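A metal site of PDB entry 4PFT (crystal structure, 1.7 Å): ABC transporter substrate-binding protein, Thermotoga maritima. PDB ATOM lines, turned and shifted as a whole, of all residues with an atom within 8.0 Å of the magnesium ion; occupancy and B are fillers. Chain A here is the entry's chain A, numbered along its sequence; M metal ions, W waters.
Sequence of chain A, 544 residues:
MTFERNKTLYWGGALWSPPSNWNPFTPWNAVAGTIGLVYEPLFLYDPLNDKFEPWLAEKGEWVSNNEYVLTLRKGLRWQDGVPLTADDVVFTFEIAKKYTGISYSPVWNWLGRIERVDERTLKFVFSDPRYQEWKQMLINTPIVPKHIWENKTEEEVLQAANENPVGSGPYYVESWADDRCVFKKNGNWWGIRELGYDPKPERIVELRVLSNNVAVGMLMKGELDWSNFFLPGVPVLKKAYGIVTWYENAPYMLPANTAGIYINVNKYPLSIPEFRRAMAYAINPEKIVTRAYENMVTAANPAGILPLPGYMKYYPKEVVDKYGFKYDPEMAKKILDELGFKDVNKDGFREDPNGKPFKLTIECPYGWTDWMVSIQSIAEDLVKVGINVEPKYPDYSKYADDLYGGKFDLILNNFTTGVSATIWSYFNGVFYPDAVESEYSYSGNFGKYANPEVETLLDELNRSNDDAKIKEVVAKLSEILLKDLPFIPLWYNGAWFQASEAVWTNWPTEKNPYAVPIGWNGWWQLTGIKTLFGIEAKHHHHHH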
ATOM      1  N   LYS A 342     -26.670  -9.342 -27.259  1.00  0.00           N
ATOM      2  CA  LYS A 342     -27.810  -9.616 -28.126  1.00  0.00           C
ATOM      3  C   LYS A 342     -28.599  -8.347 -28.394  1.00  0.00           C
ATOM      4  O   LYS A 342     -28.688  -7.464 -27.538  1.00  0.00           O
ATOM      5  CB  LYS A 342     -28.714 -10.692 -27.494  1.00  0.00           C
ATOM      6  CG  LYS A 342     -28.003 -12.043 -27.340  1.00  0.00           C
ATOM      7  CD  LYS A 342     -28.911 -13.125 -26.808  1.00  0.00           C
ATOM      8  CE  LYS A 342     -28.158 -14.440 -26.652  1.00  0.00           C
ATOM      9  NZ  LYS A 342     -29.038 -15.534 -26.170  1.00  0.00           N
ATOM     10  N   ASP A 343     -29.165  -8.256 -29.599  1.00  0.00           N
ATOM     11  CA  ASP A 343     -30.010  -7.130 -29.995  1.00  0.00           C
ATOM     12  C   ASP A 343     -31.467  -7.318 -29.555  1.00  0.00           C
ATOM     13  O   ASP A 343     -32.336  -7.659 -30.363  1.00  0.00           O
ATOM     14  CB  ASP A 343     -29.944  -6.965 -31.511  1.00  0.00           C
ATOM     15  CG  ASP A 343     -30.768  -5.823 -32.012  1.00  0.00           C
ATOM     16  OD1 ASP A 343     -30.875  -4.806 -31.294  1.00  0.00           O
ATOM     17  OD2 ASP A 343     -31.332  -5.959 -33.125  1.00  0.00           O
ATOM     18  N   VAL A 344     -31.722  -7.098 -28.270  1.00  0.00           N
ATOM     19  CA  VAL A 344     -33.039  -7.341 -27.711  1.00  0.00           C
ATOM     20  C   VAL A 344     -34.040  -6.314 -28.233  1.00  0.00           C
ATOM     21  O   VAL A 344     -35.200  -6.647 -28.464  1.00  0.00           O
ATOM     22  CB  VAL A 344     -32.992  -7.320 -26.169  1.00  0.00           C
ATOM     23  CG1 VAL A 344     -34.390  -7.504 -25.592  1.00  0.00           C
ATOM     24  CG2 VAL A 344     -32.071  -8.410 -25.662  1.00  0.00           C
ATOM     25  N   ASN A 345     -33.578  -5.090 -28.489  1.00  0.00           N
ATOM     26  CA  ASN A 345     -34.500  -4.021 -28.861  1.00  0.00           C
ATOM     27  C   ASN A 345     -34.719  -3.921 -30.376  1.00  0.00           C
ATOM     28  O   ASN A 345     -35.411  -3.018 -30.844  1.00  0.00           O
ATOM     29  CB  ASN A 345     -34.043  -2.681 -28.291  1.00  0.00           C
ATOM     30  CG  ASN A 345     -32.675  -2.258 -28.788  1.00  0.00           C
ATOM     31  OD1 ASN A 345     -32.174  -2.759 -29.799  1.00  0.00           O
ATOM     32  ND2 ASN A 345     -32.058  -1.313 -28.074  1.00  0.00           N
ATOM     33  N   LYS A 346     -34.140  -4.865 -31.120  1.00  0.00           N
ATOM     34  CA  LYS A 346     -34.405  -5.059 -32.551  1.00  0.00           C
ATOM     35  C   LYS A 346     -34.078  -3.849 -33.422  1.00  0.00           C
ATOM     36  O   LYS A 346     -34.793  -3.574 -34.377  1.00  0.00           O
ATOM     37  CB  LYS A 346     -35.863  -5.458 -32.770  1.00  0.00           C
ATOM     38  CG  LYS A 346     -36.338  -6.624 -31.914  1.00  0.00           C
ATOM     39  CD  LYS A 346     -35.417  -7.838 -32.028  1.00  0.00           C
ATOM     40  N   ASP A 347     -33.012  -3.126 -33.096  1.00  0.00           N
ATOM     41  CA  ASP A 347     -32.589  -1.993 -33.913  1.00  0.00           C
ATOM     42  C   ASP A 347     -31.401  -2.339 -34.805  1.00  0.00           C
ATOM     43  O   ASP A 347     -30.889  -1.482 -35.540  1.00  0.00           O
ATOM     44  CB  ASP A 347     -32.264  -0.767 -33.034  1.00  0.00           C
ATOM     45  CG  ASP A 347     -31.126  -0.999 -32.036  1.00  0.00           C
ATOM     46  OD1 ASP A 347     -30.509  -2.084 -32.033  1.00  0.00           O
ATOM     47  OD2 ASP A 347     -30.858  -0.069 -31.243  1.00  0.00           O
ATOM     48  N   GLY A 348     -30.972  -3.602 -34.764  1.00  0.00           N
ATOM     49  CA  GLY A 348     -29.873  -4.072 -35.592  1.00  0.00           C
ATOM     50  C   GLY A 348     -28.542  -4.033 -34.868  1.00  0.00           C
ATOM     51  O   GLY A 348     -27.553  -4.558 -35.377  1.00  0.00           O
ATOM     52  N   PHE A 349     -28.511  -3.391 -33.704  1.00  0.00           N
ATOM     53  CA  PHE A 349     -27.293  -3.264 -32.903  1.00  0.00           C
ATOM     54  C   PHE A 349     -27.395  -4.060 -31.611  1.00  0.00           C
ATOM     55  O   PHE A 349     -28.310  -3.859 -30.830  1.00  0.00           O
ATOM     56  CB  PHE A 349     -26.995  -1.797 -32.562  1.00  0.00           C
ATOM     57  CG  PHE A 349     -26.910  -0.907 -33.765  1.00  0.00           C
ATOM     58  CD1 PHE A 349     -25.961  -1.150 -34.744  1.00  0.00           C
ATOM     59  CD2 PHE A 349     -27.756   0.174 -33.901  1.00  0.00           C
ATOM     60  CE1 PHE A 349     -25.872  -0.338 -35.856  1.00  0.00           C
ATOM     61  CE2 PHE A 349     -27.662   0.995 -35.014  1.00  0.00           C
ATOM     62  CZ  PHE A 349     -26.732   0.739 -35.991  1.00  0.00           C
ATOM     63  N   ARG A 350     -26.440  -4.963 -31.375  1.00  0.00           N
ATOM     64  CA  ARG A 350     -26.436  -5.709 -30.128  1.00  0.00           C
ATOM     65  C   ARG A 350     -26.217  -4.784 -28.937  1.00  0.00           C
ATOM     66  O   ARG A 350     -25.436  -3.829 -29.017  1.00  0.00           O
ATOM     67  CB  ARG A 350     -25.352  -6.793 -30.182  1.00  0.00           C
ATOM     68  CG  ARG A 350     -25.647  -7.877 -31.204  1.00  0.00           C
ATOM     69  CD  ARG A 350     -24.392  -8.667 -31.544  1.00  0.00           C
ATOM     70  NE  ARG A 350     -24.671  -9.639 -32.603  1.00  0.00           N
ATOM     71  CZ  ARG A 350     -25.184 -10.854 -32.386  1.00  0.00           C
ATOM     72  NH1 ARG A 350     -25.472 -11.259 -31.153  1.00  0.00           N
ATOM     73  NH2 ARG A 350     -25.413 -11.673 -33.409  1.00  0.00           N
ATOM     74  N   GLU A 351     -26.910  -5.075 -27.842  1.00  0.00           N
ATOM     75  CA  GLU A 351     -26.637  -4.407 -26.568  1.00  0.00           C
ATOM     76  C   GLU A 351     -25.717  -5.311 -25.733  1.00  0.00           C
ATOM     77  O   GLU A 351     -25.544  -6.500 -26.057  1.00  0.00           O
ATOM     78  CB  GLU A 351     -27.936  -4.096 -25.824  1.00  0.00           C
ATOM     79  CG  GLU A 351     -28.946  -3.316 -26.656  1.00  0.00           C
ATOM     80  CD  GLU A 351     -29.939  -4.219 -27.377  1.00  0.00           C
ATOM     81  OE1 GLU A 351     -30.590  -5.060 -26.715  1.00  0.00           O
ATOM     82  OE2 GLU A 351     -30.079  -4.099 -28.608  1.00  0.00           O
ATOM     83  N   ASP A 352     -25.132  -4.759 -24.679  1.00  0.00           N
ATOM     84  CA  ASP A 352     -24.311  -5.574 -23.778  1.00  0.00           C
ATOM     85  C   ASP A 352     -25.214  -6.502 -22.954  1.00  0.00           C
ATOM     86  O   ASP A 352     -26.440  -6.433 -23.073  1.00  0.00           O
ATOM     87  CB  ASP A 352     -23.414  -4.680 -22.887  1.00  0.00           C
ATOM     88  CG  ASP A 352     -24.179  -3.868 -21.838  1.00  0.00           C
ATOM     89  OD1 ASP A 352     -25.189  -4.322 -21.263  1.00  0.00           O
ATOM     90  OD2 ASP A 352     -23.724  -2.739 -21.553  1.00  0.00           O
ATOM     91  N   GLY A 355     -28.330  -5.178 -21.241  1.00  0.00           N
ATOM     92  CA  GLY A 355     -29.322  -4.553 -22.113  1.00  0.00           C
ATOM     93  C   GLY A 355     -28.985  -3.118 -22.469  1.00  0.00           C
ATOM     94  O   GLY A 355     -29.821  -2.374 -22.974  1.00  0.00           O
ATOM     95  N   LYS A 356     -27.745  -2.721 -22.213  1.00  0.00           N
ATOM     96  CA  LYS A 356     -27.312  -1.361 -22.505  1.00  0.00           C
ATOM     97  C   LYS A 356     -26.702  -1.264 -23.901  1.00  0.00           C
ATOM     98  O   LYS A 356     -25.772  -2.003 -24.233  1.00  0.00           O
ATOM     99  CB  LYS A 356     -26.312  -0.884 -21.442  1.00  0.00           C
ATOM    100  CG  LYS A 356     -25.800   0.539 -21.658  1.00  0.00           C
ATOM    101  CD  LYS A 356     -24.632   0.822 -20.712  1.00  0.00           C
ATOM    102  CE  LYS A 356     -23.736   1.925 -21.226  1.00  0.00           C
ATOM    103  NZ  LYS A 356     -23.087   1.613 -22.538  1.00  0.00           N
ATOM    104  N   PRO A 357     -27.216  -0.347 -24.718  1.00  0.00           N
ATOM    105  CA  PRO A 357     -26.647  -0.137 -26.056  1.00  0.00           C
ATOM    106  C   PRO A 357     -25.231   0.415 -25.946  1.00  0.00           C
ATOM    107  O   PRO A 357     -24.903   1.101 -24.982  1.00  0.00           O
ATOM    108  CB  PRO A 357     -27.594   0.885 -26.702  1.00  0.00           C
ATOM    109  CG  PRO A 357     -28.795   0.936 -25.819  1.00  0.00           C
ATOM    110  CD  PRO A 357     -28.332   0.574 -24.447  1.00  0.00           C
ATOM    111  N   PHE A 358     -24.393   0.114 -26.939  1.00  0.00           N
ATOM    112  CA  PHE A 358     -23.042   0.652 -26.975  1.00  0.00           C
ATOM    113  C   PHE A 358     -22.660   0.874 -28.431  1.00  0.00           C
ATOM    114  O   PHE A 358     -23.214   0.252 -29.336  1.00  0.00           O
ATOM    115  CB  PHE A 358     -22.058  -0.303 -26.299  1.00  0.00           C
ATOM    116  CG  PHE A 358     -21.840  -1.596 -27.058  1.00  0.00           C
ATOM    117  CD1 PHE A 358     -22.758  -2.634 -26.956  1.00  0.00           C
ATOM    118  CD2 PHE A 358     -20.742  -1.753 -27.878  1.00  0.00           C
ATOM    119  CE1 PHE A 358     -22.563  -3.823 -27.656  1.00  0.00           C
ATOM    120  CE2 PHE A 358     -20.552  -2.931 -28.600  1.00  0.00           C
ATOM    121  CZ  PHE A 358     -21.473  -3.975 -28.477  1.00  0.00           C
ATOM    122  N   GLY A 386     -23.966  -6.814 -35.913  1.00  0.00           N
ATOM    123  CA  GLY A 386     -24.609  -6.136 -34.794  1.00  0.00           C
ATOM    124  C   GLY A 386     -23.727  -5.309 -33.872  1.00  0.00           C
ATOM    125  O   GLY A 386     -24.165  -4.923 -32.789  1.00  0.00           O
ATOM    126  N   ASN A 388     -22.252  -1.846 -33.350  1.00  0.00           N
ATOM    127  CA  ASN A 388     -22.347  -0.473 -33.826  1.00  0.00           C
ATOM    128  C   ASN A 388     -20.981   0.238 -33.876  1.00  0.00           C
ATOM    129  O   ASN A 388     -20.457   0.656 -32.850  1.00  0.00           O
ATOM    130  CB  ASN A 388     -23.332   0.310 -32.959  1.00  0.00           C
ATOM    131  CG  ASN A 388     -23.800   1.586 -33.627  1.00  0.00           C
ATOM    132  OD1 ASN A 388     -23.219   2.026 -34.613  1.00  0.00           O
ATOM    133  ND2 ASN A 388     -24.864   2.182 -33.082  1.00  0.00           N
HETATM  134 MG    MG M   1     -30.154  -3.105 -30.420  1.00  0.00          MG
HETATM  135  O   HOH W   1     -29.349  -1.544 -29.432  1.00  0.00           O
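Water W1 lies within hydrogen-bond range of OD2 of Asp 347 (2.8 Å) and ND2 of Asn 345 (3.0 Å).
OD1 of Asp 347 is bound to the magnesium ion, 1.9 Å away.
The magnesium ion is bound by water W1, 2.0 Å away.
The magnesium ion is bound by the backbone carbonyl oxygen (O) of Phe 349 (2.0 Å).
The magnesium ion is bound by the side-chain carboxylate (OD1) of Asp 343 (2.0 Å).
OE2 of Glu 351 binds the magnesium ion.
The magnesium ion is bound by OD1 of Asn 345 (2.1 Å).
The magnesium ion has six donor atoms within binding distance.
Five residues have an atom within 4 Å of the magnesium ion: Asp 343, Asn 345, Asp 347, Phe 349 and Glu 351.
The nearest printed residue that does not touch the magnesium ion is Arg 350 (4.3 Å).
OD1 of Asp 343 sits close to N of Lys 346 (3.3 Å).
OD2 of Asp 343 is in hydrogen-bond range of N of Gly 348, at 2.9 Å.
OE1 of Glu 351 is in hydrogen-bond range of N of Val 344.
N of Glu 351 sits at hydrogen-bond distance from O of Lys 342 (3.0 Å).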
